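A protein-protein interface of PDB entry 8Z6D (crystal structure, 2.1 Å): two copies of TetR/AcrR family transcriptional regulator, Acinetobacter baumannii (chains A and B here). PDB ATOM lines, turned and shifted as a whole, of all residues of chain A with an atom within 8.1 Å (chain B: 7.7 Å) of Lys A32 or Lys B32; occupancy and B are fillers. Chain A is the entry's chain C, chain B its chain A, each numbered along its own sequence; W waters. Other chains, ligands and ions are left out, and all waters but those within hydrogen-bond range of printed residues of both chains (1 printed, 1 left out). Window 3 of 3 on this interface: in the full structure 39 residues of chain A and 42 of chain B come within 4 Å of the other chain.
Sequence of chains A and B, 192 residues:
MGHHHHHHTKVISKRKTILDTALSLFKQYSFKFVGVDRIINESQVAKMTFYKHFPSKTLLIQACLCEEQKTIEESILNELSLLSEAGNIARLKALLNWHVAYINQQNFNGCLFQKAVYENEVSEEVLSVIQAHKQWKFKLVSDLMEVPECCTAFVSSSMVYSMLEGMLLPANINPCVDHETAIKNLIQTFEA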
ATOM      1  N   PHE A  26      11.605 -14.976  -8.229  1.00  0.00           N
ATOM      2  CA  PHE A  26      11.444 -15.702  -6.970  1.00  0.00           C
ATOM      3  C   PHE A  26       9.999 -16.151  -6.758  1.00  0.00           C
ATOM      4  O   PHE A  26       9.752 -17.227  -6.192  1.00  0.00           O
ATOM      5  CB  PHE A  26      11.889 -14.833  -5.794  1.00  0.00           C
ATOM      6  CG  PHE A  26      13.381 -14.593  -5.719  1.00  0.00           C
ATOM      7  CD1 PHE A  26      14.289 -15.588  -6.049  1.00  0.00           C
ATOM      8  CD2 PHE A  26      13.869 -13.367  -5.294  1.00  0.00           C
ATOM      9  CE1 PHE A  26      15.648 -15.366  -5.965  1.00  0.00           C
ATOM     10  CE2 PHE A  26      15.239 -13.131  -5.208  1.00  0.00           C
ATOM     11  CZ  PHE A  26      16.131 -14.134  -5.550  1.00  0.00           C
ATOM     12  N   TYR A  29       9.138 -19.052  -9.359  1.00  0.00           N
ATOM     13  CA  TYR A  29       9.767 -20.297  -8.952  1.00  0.00           C
ATOM     14  C   TYR A  29       9.939 -20.351  -7.436  1.00  0.00           C
ATOM     15  O   TYR A  29       8.958 -20.484  -6.696  1.00  0.00           O
ATOM     16  CB  TYR A  29      11.116 -20.452  -9.657  1.00  0.00           C
ATOM     17  CG  TYR A  29      11.077 -20.322 -11.177  1.00  0.00           C
ATOM     18  CD1 TYR A  29      10.455 -21.291 -11.971  1.00  0.00           C
ATOM     19  CD2 TYR A  29      11.677 -19.246 -11.823  1.00  0.00           C
ATOM     20  CE1 TYR A  29      10.433 -21.183 -13.366  1.00  0.00           C
ATOM     21  CE2 TYR A  29      11.655 -19.131 -13.215  1.00  0.00           C
ATOM     22  CZ  TYR A  29      11.036 -20.104 -13.978  1.00  0.00           C
ATOM     23  OH  TYR A  29      11.018 -19.995 -15.352  1.00  0.00           O
ATOM     24  N   SER A  30      11.182 -20.249  -6.968  1.00  0.00           N
ATOM     25  CA  SER A  30      11.482 -20.235  -5.545  1.00  0.00           C
ATOM     26  C   SER A  30      12.826 -19.542  -5.335  1.00  0.00           C
ATOM     27  O   SER A  30      13.653 -19.455  -6.246  1.00  0.00           O
ATOM     28  CB  SER A  30      11.478 -21.657  -4.956  1.00  0.00           C
ATOM     29  OG  SER A  30      12.748 -22.292  -5.032  1.00  0.00           O
ATOM     30  N   PHE A  31      13.020 -19.034  -4.114  1.00  0.00           N
ATOM     31  CA  PHE A  31      14.265 -18.353  -3.775  1.00  0.00           C
ATOM     32  C   PHE A  31      15.464 -19.244  -4.047  1.00  0.00           C
ATOM     33  O   PHE A  31      16.462 -18.803  -4.634  1.00  0.00           O
ATOM     34  CB  PHE A  31      14.251 -17.917  -2.311  1.00  0.00           C
ATOM     35  CG  PHE A  31      13.374 -16.720  -2.041  1.00  0.00           C
ATOM     36  CD1 PHE A  31      13.734 -15.460  -2.499  1.00  0.00           C
ATOM     37  CD2 PHE A  31      12.198 -16.857  -1.319  1.00  0.00           C
ATOM     38  CE1 PHE A  31      12.932 -14.360  -2.249  1.00  0.00           C
ATOM     39  CE2 PHE A  31      11.402 -15.766  -1.056  1.00  0.00           C
ATOM     40  CZ  PHE A  31      11.759 -14.514  -1.531  1.00  0.00           C
ATOM     41  N   LYS A  32      15.378 -20.510  -3.631  1.00  0.00           N
ATOM     42  CA  LYS A  32      16.489 -21.430  -3.836  1.00  0.00           C
ATOM     43  C   LYS A  32      16.665 -21.759  -5.316  1.00  0.00           C
ATOM     44  O   LYS A  32      17.796 -21.895  -5.798  1.00  0.00           O
ATOM     45  CB  LYS A  32      16.261 -22.700  -3.016  1.00  0.00           C
ATOM     46  CG  LYS A  32      17.431 -23.664  -3.047  1.00  0.00           C
ATOM     47  CD  LYS A  32      18.668 -23.001  -2.472  1.00  0.00           C
ATOM     48  CE  LYS A  32      19.508 -23.998  -1.700  1.00  0.00           C
ATOM     49  NZ  LYS A  32      19.606 -25.280  -2.454  1.00  0.00           N
ATOM     50  N   PHE A  33      15.558 -21.875  -6.052  1.00  0.00           N
ATOM     51  CA  PHE A  33      15.619 -22.316  -7.439  1.00  0.00           C
ATOM     52  C   PHE A  33      16.235 -21.271  -8.364  1.00  0.00           C
ATOM     53  O   PHE A  33      16.735 -21.632  -9.437  1.00  0.00           O
ATOM     54  CB  PHE A  33      14.217 -22.688  -7.938  1.00  0.00           C
ATOM     55  CG  PHE A  33      14.230 -23.453  -9.234  1.00  0.00           C
ATOM     56  CD1 PHE A  33      15.252 -24.356  -9.507  1.00  0.00           C
ATOM     57  CD2 PHE A  33      13.256 -23.241 -10.199  1.00  0.00           C
ATOM     58  CE1 PHE A  33      15.286 -25.054 -10.704  1.00  0.00           C
ATOM     59  CE2 PHE A  33      13.281 -23.940 -11.407  1.00  0.00           C
ATOM     60  CZ  PHE A  33      14.301 -24.846 -11.655  1.00  0.00           C
ATOM     61  N   VAL A  34      16.199 -19.994  -7.986  1.00  0.00           N
ATOM     62  CA  VAL A  34      16.683 -18.904  -8.827  1.00  0.00           C
ATOM     63  C   VAL A  34      18.058 -18.494  -8.334  1.00  0.00           C
ATOM     64  O   VAL A  34      18.198 -18.035  -7.197  1.00  0.00           O
ATOM     65  CB  VAL A  34      15.726 -17.702  -8.800  1.00  0.00           C
ATOM     66  CG1 VAL A  34      16.271 -16.592  -9.693  1.00  0.00           C
ATOM     67  CG2 VAL A  34      14.306 -18.115  -9.205  1.00  0.00           C
ATOM     68  N   GLY A  35      19.072 -18.639  -9.197  1.00  0.00           N
ATOM     69  CA  GLY A  35      20.427 -18.289  -8.838  1.00  0.00           C
ATOM     70  C   GLY A  35      20.792 -16.862  -9.205  1.00  0.00           C
ATOM     71  O   GLY A  35      20.203 -16.244 -10.094  1.00  0.00           O
ATOM     72  N   VAL A  36      21.785 -16.337  -8.489  1.00  0.00           N
ATOM     73  CA  VAL A  36      22.174 -14.943  -8.675  1.00  0.00           C
ATOM     74  C   VAL A  36      22.543 -14.693 -10.123  1.00  0.00           C
ATOM     75  O   VAL A  36      22.195 -13.654 -10.699  1.00  0.00           O
ATOM     76  CB  VAL A  36      23.325 -14.575  -7.719  1.00  0.00           C
ATOM     77  CG1 VAL A  36      24.127 -13.398  -8.260  1.00  0.00           C
ATOM     78  CG2 VAL A  36      22.776 -14.249  -6.336  1.00  0.00           C
ATOM     79  N   LYS A  57      23.263 -12.799  -2.188  1.00  0.00           N
ATOM     80  CA  LYS A  57      21.884 -13.171  -2.484  1.00  0.00           C
ATOM     81  C   LYS A  57      20.966 -12.885  -1.304  1.00  0.00           C
ATOM     82  O   LYS A  57      19.784 -12.586  -1.499  1.00  0.00           O
ATOM     83  CB  LYS A  57      21.806 -14.648  -2.866  1.00  0.00           C
ATOM     84  CG  LYS A  57      20.427 -15.099  -3.333  1.00  0.00           C
ATOM     85  CD  LYS A  57      20.465 -16.553  -3.759  1.00  0.00           C
ATOM     86  CE  LYS A  57      19.153 -16.974  -4.427  1.00  0.00           C
ATOM     87  NZ  LYS A  57      19.096 -18.459  -4.617  1.00  0.00           N
ATOM     88  N   ILE A  61      17.570 -10.756  -1.442  1.00  0.00           N
ATOM     89  CA  ILE A  61      16.296 -11.297  -0.978  1.00  0.00           C
ATOM     90  C   ILE A  61      15.675 -10.378   0.066  1.00  0.00           C
ATOM     91  O   ILE A  61      14.464 -10.150   0.065  1.00  0.00           O
ATOM     92  CB  ILE A  61      16.490 -12.725  -0.433  1.00  0.00           C
ATOM     93  CG1 ILE A  61      16.668 -13.723  -1.580  1.00  0.00           C
ATOM     94  CG2 ILE A  61      15.324 -13.131   0.451  1.00  0.00           C
ATOM     95  CD1 ILE A  61      17.116 -15.115  -1.116  1.00  0.00           C
ATOM     96  N   LYS A 115       6.694 -18.324   1.792  1.00  0.00           N
ATOM     97  CA  LYS A 115       7.662 -19.067   0.985  1.00  0.00           C
ATOM     98  C   LYS A 115       9.087 -18.889   1.502  1.00  0.00           C
ATOM     99  O   LYS A 115       9.831 -19.865   1.649  1.00  0.00           O
ATOM    100  CB  LYS A 115       7.574 -18.623  -0.478  1.00  0.00           C
ATOM    101  CG  LYS A 115       8.770 -19.057  -1.293  1.00  0.00           C
ATOM    102  CD  LYS A 115       8.515 -19.227  -2.777  1.00  0.00           C
ATOM    103  CE  LYS A 115       7.394 -18.376  -3.297  1.00  0.00           C
ATOM    104  NZ  LYS A 115       7.122 -18.728  -4.725  1.00  0.00           N
ATOM    105  N   ALA A 116       9.489 -17.642   1.778  1.00  0.00           N
ATOM    106  CA  ALA A 116      10.851 -17.387   2.251  1.00  0.00           C
ATOM    107  C   ALA A 116      11.145 -18.171   3.523  1.00  0.00           C
ATOM    108  O   ALA A 116      12.199 -18.809   3.644  1.00  0.00           O
ATOM    109  CB  ALA A 116      11.062 -15.888   2.495  1.00  0.00           C
ATOM    110  N   TYR A 118       9.665 -20.876   4.734  1.00  0.00           N
ATOM    111  CA  TYR A 118       9.649 -22.317   4.480  1.00  0.00           C
ATOM    112  C   TYR A 118      10.871 -22.788   3.705  1.00  0.00           C
ATOM    113  O   TYR A 118      11.209 -23.978   3.771  1.00  0.00           O
ATOM    114  CB  TYR A 118       8.377 -22.703   3.728  1.00  0.00           C
ATOM    115  CG  TYR A 118       7.232 -23.096   4.634  1.00  0.00           C
ATOM    116  CD1 TYR A 118       7.417 -24.020   5.651  1.00  0.00           C
ATOM    117  CD2 TYR A 118       5.971 -22.544   4.472  1.00  0.00           C
ATOM    118  CE1 TYR A 118       6.391 -24.380   6.483  1.00  0.00           C
ATOM    119  CE2 TYR A 118       4.925 -22.907   5.303  1.00  0.00           C
ATOM    120  CZ  TYR A 118       5.146 -23.820   6.297  1.00  0.00           C
ATOM    121  OH  TYR A 118       4.114 -24.184   7.111  1.00  0.00           O
ATOM    122  N   GLU A 119      11.524 -21.892   2.961  1.00  0.00           N
ATOM    123  CA  GLU A 119      12.761 -22.197   2.253  1.00  0.00           C
ATOM    124  C   GLU A 119      13.983 -21.956   3.126  1.00  0.00           C
ATOM    125  O   GLU A 119      15.118 -21.958   2.623  1.00  0.00           O
ATOM    126  CB  GLU A 119      12.856 -21.373   0.972  1.00  0.00           C
ATOM    127  CG  GLU A 119      11.880 -21.814  -0.106  1.00  0.00           C
ATOM    128  CD  GLU A 119      12.309 -21.412  -1.507  1.00  0.00           C
ATOM    129  OE1 GLU A 119      13.185 -22.095  -2.075  1.00  0.00           O
ATOM    130  OE2 GLU A 119      11.767 -20.425  -2.047  1.00  0.00           O
ATOM    131  N   ASN A 120      13.759 -21.730   4.419  1.00  0.00           N
ATOM    132  CA  ASN A 120      14.810 -21.620   5.407  1.00  0.00           C
ATOM    133  C   ASN A 120      15.658 -20.362   5.204  1.00  0.00           C
ATOM    134  O   ASN A 120      16.853 -20.353   5.505  1.00  0.00           O
ATOM    135  CB  ASN A 120      15.686 -22.874   5.409  1.00  0.00           C
ATOM    136  CG  ASN A 120      16.405 -23.065   6.710  1.00  0.00           C
ATOM    137  OD1 ASN A 120      15.792 -23.049   7.784  1.00  0.00           O
ATOM    138  ND2 ASN A 120      17.718 -23.224   6.634  1.00  0.00           N
ATOM    139  N   GLU A 121      15.037 -19.300   4.695  1.00  0.00           N
ATOM    140  CA  GLU A 121      15.624 -17.958   4.687  1.00  0.00           C
ATOM    141  C   GLU A 121      15.412 -17.340   6.071  1.00  0.00           C
ATOM    142  O   GLU A 121      14.488 -16.550   6.312  1.00  0.00           O
ATOM    143  CB  GLU A 121      14.999 -17.109   3.581  1.00  0.00           C
ATOM    144  CG  GLU A 121      15.410 -17.549   2.154  1.00  0.00           C
ATOM    145  CD  GLU A 121      16.893 -17.292   1.858  1.00  0.00           C
ATOM    146  OE1 GLU A 121      17.508 -16.428   2.529  1.00  0.00           O
ATOM    147  OE2 GLU A 121      17.459 -17.942   0.955  1.00  0.00           O
ATOM    148  N   PHE B  26      14.551 -32.491   7.013  1.00  0.00           N
ATOM    149  CA  PHE B  26      13.587 -31.744   6.211  1.00  0.00           C
ATOM    150  C   PHE B  26      12.712 -30.852   7.079  1.00  0.00           C
ATOM    151  O   PHE B  26      12.444 -29.698   6.724  1.00  0.00           O
ATOM    152  CB  PHE B  26      12.719 -32.712   5.407  1.00  0.00           C
ATOM    153  CG  PHE B  26      13.486 -33.468   4.352  1.00  0.00           C
ATOM    154  CD1 PHE B  26      14.582 -32.892   3.742  1.00  0.00           C
ATOM    155  CD2 PHE B  26      13.112 -34.749   3.973  1.00  0.00           C
ATOM    156  CE1 PHE B  26      15.287 -33.575   2.765  1.00  0.00           C
ATOM    157  CE2 PHE B  26      13.806 -35.438   2.996  1.00  0.00           C
ATOM    158  CZ  PHE B  26      14.896 -34.856   2.388  1.00  0.00           C
ATOM    159  N   TYR B  29      15.081 -27.939   8.540  1.00  0.00           N
ATOM    160  CA  TYR B  29      15.602 -26.964   7.598  1.00  0.00           C
ATOM    161  C   TYR B  29      14.615 -26.866   6.450  1.00  0.00           C
ATOM    162  O   TYR B  29      13.592 -26.185   6.573  1.00  0.00           O
ATOM    163  CB  TYR B  29      17.021 -27.340   7.170  1.00  0.00           C
ATOM    164  CG  TYR B  29      17.962 -27.539   8.334  1.00  0.00           C
ATOM    165  CD1 TYR B  29      18.426 -26.451   9.080  1.00  0.00           C
ATOM    166  CD2 TYR B  29      18.374 -28.816   8.708  1.00  0.00           C
ATOM    167  CE1 TYR B  29      19.292 -26.636  10.162  1.00  0.00           C
ATOM    168  CE2 TYR B  29      19.237 -29.012   9.785  1.00  0.00           C
ATOM    169  CZ  TYR B  29      19.690 -27.922  10.509  1.00  0.00           C
ATOM    170  OH  TYR B  29      20.539 -28.135  11.579  1.00  0.00           O
ATOM    171  N   SER B  30      14.875 -27.519   5.320  1.00  0.00           N
ATOM    172  CA  SER B  30      13.930 -27.573   4.212  1.00  0.00           C
ATOM    173  C   SER B  30      14.337 -28.732   3.315  1.00  0.00           C
ATOM    174  O   SER B  30      15.392 -29.336   3.505  1.00  0.00           O
ATOM    175  CB  SER B  30      13.884 -26.247   3.441  1.00  0.00           C
ATOM    176  OG  SER B  30      14.938 -26.192   2.491  1.00  0.00           O
ATOM    177  N   PHE B  31      13.473 -29.057   2.346  1.00  0.00           N
ATOM    178  CA  PHE B  31      13.792 -30.145   1.417  1.00  0.00           C
ATOM    179  C   PHE B  31      15.012 -29.807   0.551  1.00  0.00           C
ATOM    180  O   PHE B  31      15.959 -30.594   0.464  1.00  0.00           O
ATOM    181  CB  PHE B  31      12.581 -30.467   0.536  1.00  0.00           C
ATOM    182  CG  PHE B  31      11.416 -31.045   1.285  1.00  0.00           C
ATOM    183  CD1 PHE B  31      11.450 -32.345   1.753  1.00  0.00           C
ATOM    184  CD2 PHE B  31      10.276 -30.275   1.533  1.00  0.00           C
ATOM    185  CE1 PHE B  31      10.371 -32.874   2.442  1.00  0.00           C
ATOM    186  CE2 PHE B  31       9.186 -30.806   2.220  1.00  0.00           C
ATOM    187  CZ  PHE B  31       9.244 -32.109   2.675  1.00  0.00           C
ATOM    188  N   LYS B  32      15.011 -28.637  -0.094  1.00  0.00           N
ATOM    189  CA  LYS B  32      16.107 -28.284  -0.994  1.00  0.00           C
ATOM    190  C   LYS B  32      17.397 -27.988  -0.246  1.00  0.00           C
ATOM    191  O   LYS B  32      18.470 -28.028  -0.846  1.00  0.00           O
ATOM    192  CB  LYS B  32      15.745 -27.070  -1.849  1.00  0.00           C
ATOM    193  CG  LYS B  32      15.295 -27.397  -3.266  1.00  0.00           C
ATOM    194  CD  LYS B  32      13.981 -26.689  -3.604  1.00  0.00           C
ATOM    195  CE  LYS B  32      13.466 -27.087  -4.990  1.00  0.00           C
ATOM    196  NZ  LYS B  32      13.116 -28.539  -5.060  1.00  0.00           N
ATOM    197  N   PHE B  33      17.314 -27.698   1.047  1.00  0.00           N
ATOM    198  CA  PHE B  33      18.492 -27.277   1.786  1.00  0.00           C
ATOM    199  C   PHE B  33      19.326 -28.468   2.238  1.00  0.00           C
ATOM    200  O   PHE B  33      20.549 -28.346   2.351  1.00  0.00           O
ATOM    201  CB  PHE B  33      18.071 -26.395   2.974  1.00  0.00           C
ATOM    202  CG  PHE B  33      19.214 -25.991   3.880  1.00  0.00           C
ATOM    203  CD1 PHE B  33      19.609 -26.807   4.939  1.00  0.00           C
ATOM    204  CD2 PHE B  33      19.888 -24.801   3.675  1.00  0.00           C
ATOM    205  CE1 PHE B  33      20.664 -26.446   5.777  1.00  0.00           C
ATOM    206  CE2 PHE B  33      20.956 -24.434   4.502  1.00  0.00           C
ATOM    207  CZ  PHE B  33      21.338 -25.260   5.555  1.00  0.00           C
ATOM    208  N   VAL B  34      18.715 -29.623   2.499  1.00  0.00           N
ATOM    209  CA  VAL B  34      19.480 -30.791   2.924  1.00  0.00           C
ATOM    210  C   VAL B  34      19.566 -31.761   1.750  1.00  0.00           C
ATOM    211  O   VAL B  34      18.544 -32.234   1.234  1.00  0.00           O
ATOM    212  CB  VAL B  34      18.905 -31.441   4.200  1.00  0.00           C
ATOM    213  CG1 VAL B  34      17.719 -30.692   4.713  1.00  0.00           C
ATOM    214  CG2 VAL B  34      18.625 -32.943   4.043  1.00  0.00           C
ATOM    215  N   GLY B  35      20.812 -31.996   1.285  1.00  0.00           N
ATOM    216  CA  GLY B  35      21.072 -32.913   0.196  1.00  0.00           C
ATOM    217  C   GLY B  35      21.215 -34.341   0.674  1.00  0.00           C
ATOM    218  O   GLY B  35      21.266 -34.620   1.870  1.00  0.00           O
ATOM    219  N   LYS B  57      16.072 -38.961  -4.470  1.00  0.00           N
ATOM    220  CA  LYS B  57      15.670 -38.057  -3.402  1.00  0.00           C
ATOM    221  C   LYS B  57      14.168 -37.797  -3.427  1.00  0.00           C
ATOM    222  O   LYS B  57      13.542 -37.659  -2.373  1.00  0.00           O
ATOM    223  CB  LYS B  57      16.436 -36.735  -3.498  1.00  0.00           C
ATOM    224  CG  LYS B  57      16.217 -35.856  -2.262  1.00  0.00           C
ATOM    225  CD  LYS B  57      16.986 -34.557  -2.323  1.00  0.00           C
ATOM    226  CE  LYS B  57      16.782 -33.741  -1.054  1.00  0.00           C
ATOM    227  NZ  LYS B  57      16.960 -32.298  -1.354  1.00  0.00           N
ATOM    228  N   ILE B  61      11.533 -38.190  -0.441  1.00  0.00           N
ATOM    229  CA  ILE B  61      10.607 -37.114  -0.088  1.00  0.00           C
ATOM    230  C   ILE B  61       9.173 -37.629  -0.100  1.00  0.00           C
ATOM    231  O   ILE B  61       8.399 -37.353   0.822  1.00  0.00           O
ATOM    232  CB  ILE B  61      10.787 -35.898  -1.016  1.00  0.00           C
ATOM    233  CG1 ILE B  61      12.078 -35.163  -0.663  1.00  0.00           C
ATOM    234  CG2 ILE B  61       9.615 -34.949  -0.868  1.00  0.00           C
ATOM    235  CD1 ILE B  61      12.385 -33.997  -1.581  1.00  0.00           C
ATOM    236  N   LYS B 115       5.326 -26.748   3.363  1.00  0.00           N
ATOM    237  CA  LYS B 115       6.715 -26.576   2.956  1.00  0.00           C
ATOM    238  C   LYS B 115       6.966 -27.183   1.575  1.00  0.00           C
ATOM    239  O   LYS B 115       7.648 -26.580   0.743  1.00  0.00           O
ATOM    240  CB  LYS B 115       7.672 -27.196   3.987  1.00  0.00           C
ATOM    241  CG  LYS B 115       9.127 -26.803   3.737  1.00  0.00           C
ATOM    242  CD  LYS B 115      10.147 -27.674   4.462  1.00  0.00           C
ATOM    243  CE  LYS B 115      10.199 -27.399   5.962  1.00  0.00           C
ATOM    244  NZ  LYS B 115      10.827 -26.066   6.251  1.00  0.00           N
ATOM    245  N   ALA B 116       6.433 -28.382   1.315  1.00  0.00           N
ATOM    246  CA  ALA B 116       6.707 -29.029   0.036  1.00  0.00           C
ATOM    247  C   ALA B 116       6.125 -28.227  -1.123  1.00  0.00           C
ATOM    248  O   ALA B 116       6.756 -28.117  -2.180  1.00  0.00           O
ATOM    249  CB  ALA B 116       6.174 -30.466   0.044  1.00  0.00           C
ATOM    250  N   TYR B 118       5.597 -24.913  -1.175  1.00  0.00           N
ATOM    251  CA  TYR B 118       6.329 -23.656  -1.340  1.00  0.00           C
ATOM    252  C   TYR B 118       7.690 -23.884  -1.984  1.00  0.00           C
ATOM    253  O   TYR B 118       8.158 -23.035  -2.744  1.00  0.00           O
ATOM    254  CB  TYR B 118       6.489 -22.929  -0.008  1.00  0.00           C
ATOM    255  CG  TYR B 118       5.349 -21.960   0.287  1.00  0.00           C
ATOM    256  CD1 TYR B 118       5.033 -20.931  -0.600  1.00  0.00           C
ATOM    257  CD2 TYR B 118       4.566 -22.098   1.435  1.00  0.00           C
ATOM    258  CE1 TYR B 118       3.973 -20.043  -0.339  1.00  0.00           C
ATOM    259  CE2 TYR B 118       3.502 -21.225   1.707  1.00  0.00           C
ATOM    260  CZ  TYR B 118       3.224 -20.195   0.819  1.00  0.00           C
ATOM    261  OH  TYR B 118       2.186 -19.342   1.086  1.00  0.00           O
ATOM    262  N   GLU B 119       8.316 -25.029  -1.718  1.00  0.00           N
ATOM    263  CA  GLU B 119       9.568 -25.442  -2.335  1.00  0.00           C
ATOM    264  C   GLU B 119       9.375 -26.106  -3.687  1.00  0.00           C
ATOM    265  O   GLU B 119      10.362 -26.480  -4.329  1.00  0.00           O
ATOM    266  CB  GLU B 119      10.311 -26.385  -1.385  1.00  0.00           C
ATOM    267  CG  GLU B 119      10.785 -25.676  -0.149  1.00  0.00           C
ATOM    268  CD  GLU B 119      11.858 -26.433   0.554  1.00  0.00           C
ATOM    269  OE1 GLU B 119      13.040 -26.331   0.145  1.00  0.00           O
ATOM    270  OE2 GLU B 119      11.519 -27.136   1.522  1.00  0.00           O
ATOM    271  N   ASN B 120       8.138 -26.253  -4.144  1.00  0.00           N
ATOM    272  CA  ASN B 120       7.857 -26.833  -5.453  1.00  0.00           C
ATOM    273  C   ASN B 120       8.343 -28.283  -5.544  1.00  0.00           C
ATOM    274  O   ASN B 120       8.722 -28.757  -6.619  1.00  0.00           O
ATOM    275  CB  ASN B 120       8.444 -25.976  -6.582  1.00  0.00           C
ATOM    276  CG  ASN B 120       7.405 -25.047  -7.177  1.00  0.00           C
ATOM    277  OD1 ASN B 120       7.452 -23.818  -6.986  1.00  0.00           O
ATOM    278  ND2 ASN B 120       6.413 -25.639  -7.858  1.00  0.00           N
ATOM    279  N   GLU B 121       8.338 -28.981  -4.406  1.00  0.00           N
ATOM    280  CA  GLU B 121       8.397 -30.441  -4.355  1.00  0.00           C
ATOM    281  C   GLU B 121       7.012 -30.985  -4.711  1.00  0.00           C
ATOM    282  O   GLU B 121       6.195 -31.338  -3.858  1.00  0.00           O
ATOM    283  CB  GLU B 121       8.846 -30.910  -2.978  1.00  0.00           C
ATOM    284  CG  GLU B 121      10.265 -30.517  -2.627  1.00  0.00           C
ATOM    285  CD  GLU B 121      11.312 -31.076  -3.606  1.00  0.00           C
ATOM    286  OE1 GLU B 121      11.042 -32.066  -4.331  1.00  0.00           O
ATOM    287  OE2 GLU B 121      12.418 -30.512  -3.648  1.00  0.00           O
ATOM    288  N   VAL B 122       6.726 -31.026  -6.005  1.00  0.00           N
ATOM    289  CA  VAL B 122       5.357 -31.307  -6.407  1.00  0.00           C
ATOM    290  C   VAL B 122       5.307 -32.283  -7.567  1.00  0.00           C
ATOM    291  O   VAL B 122       4.383 -32.223  -8.378  1.00  0.00           O
ATOM    292  CB  VAL B 122       4.604 -30.012  -6.771  1.00  0.00           C
ATOM    293  CG1 VAL B 122       4.373 -29.141  -5.511  1.00  0.00           C
ATOM    294  CG2 VAL B 122       5.336 -29.261  -7.875  1.00  0.00           C
HETATM  295  O   HOH W   1      13.090 -23.758   8.247  1.00  0.00           O
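Printed residues of chain B that touch a printed residue of chain A: Tyr B29, Ser B30, Lys B32, Phe B33, Lys B115, Tyr B118, Glu B119 and Asn B120.
Of the 17 printed residues of chain A, 5 touch a printed residue of chain B.
Printed residues of chain A that touch a printed residue of chain B: Tyr A29, Lys A32, Lys A115, Tyr A118 and Asn A120.
Among the printed residues, merely in contact across the chains: Tyr A29 with Asn B120, Lys A115 with Tyr B118, Tyr A118 with Ser B30, Tyr A118 with Tyr B118, Tyr A118 with Glu B119, Asn A120 with Tyr B29 and Asn A120 with Phe B33.
NZ of Lys B115 is in hydrogen-bond range of O of Tyr B29 (2.8 Å).
The side-chain carboxylate (OE1) of Glu B119 lies within hydrogen-bond range of the side-chain hydroxyl (OG) of Ser B30, 3.0 Å away.
The backbone NH (N) of Phe B31 is in hydrogen-bond range of the side-chain carboxylate (OE2) of Glu B119 (2.9 Å).
The side-chain carboxylate (OE2) of Glu B121 is in salt-bridge range of the side-chain amino group (NZ) of Lys B32 (2.5 Å).
The side-chain hydroxyl of Ser A30 lies close to the backbone NH of Lys A32 (3.5 Å).
The backbone NH of Lys A32 sits at hydrogen-bond distance from the side-chain carboxylate of Glu A119 (3.1 Å).
Lys A32 touches its own counterpart, Lys B32.
Tyr B118 touches its own counterpart, Tyr A118.
Tyr A118 touches Glu B119, but with the chains exchanged Glu A119 does not touch Tyr B118 (4.5 Å).
Asn A120 touches Phe B33, but with the chains exchanged Phe A33 does not touch Asn B120 (6.6 Å).
16 positions are printed for both chains.
Of the 9 pairs that touch across the chains among the printed residues, 6 have their exchanged pair printed and touching as well.
Water W1 lies within hydrogen-bond range of OD1 of Asn A120 and O of Tyr B29.
Printed residues of chain B within 4 Å of Lys A115: Tyr B118.
Phe B31 touches none of the printed residues of chain A.
Of the printed residues of chain A, Phe B33 touches Asn A120 (3.99 Å).
Lys B57 touches none of the printed residues of chain A.
Printed residues of chain A within 4 Å of Lys B115: Tyr A118 (3.3 Å).
Printed residues of chain A within 4 Å of Glu B119: Tyr A118.
Of the printed residues of chain A, Asn B120 touches Tyr A29.
O of Lys B32 is in hydrogen-bond range of NZ of Lys A32 (3.4 Å).
The backbone carbonyl oxygen of Tyr A118 sits at hydrogen-bond distance from the side-chain amino group of Lys B115, 3.3 Å away.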
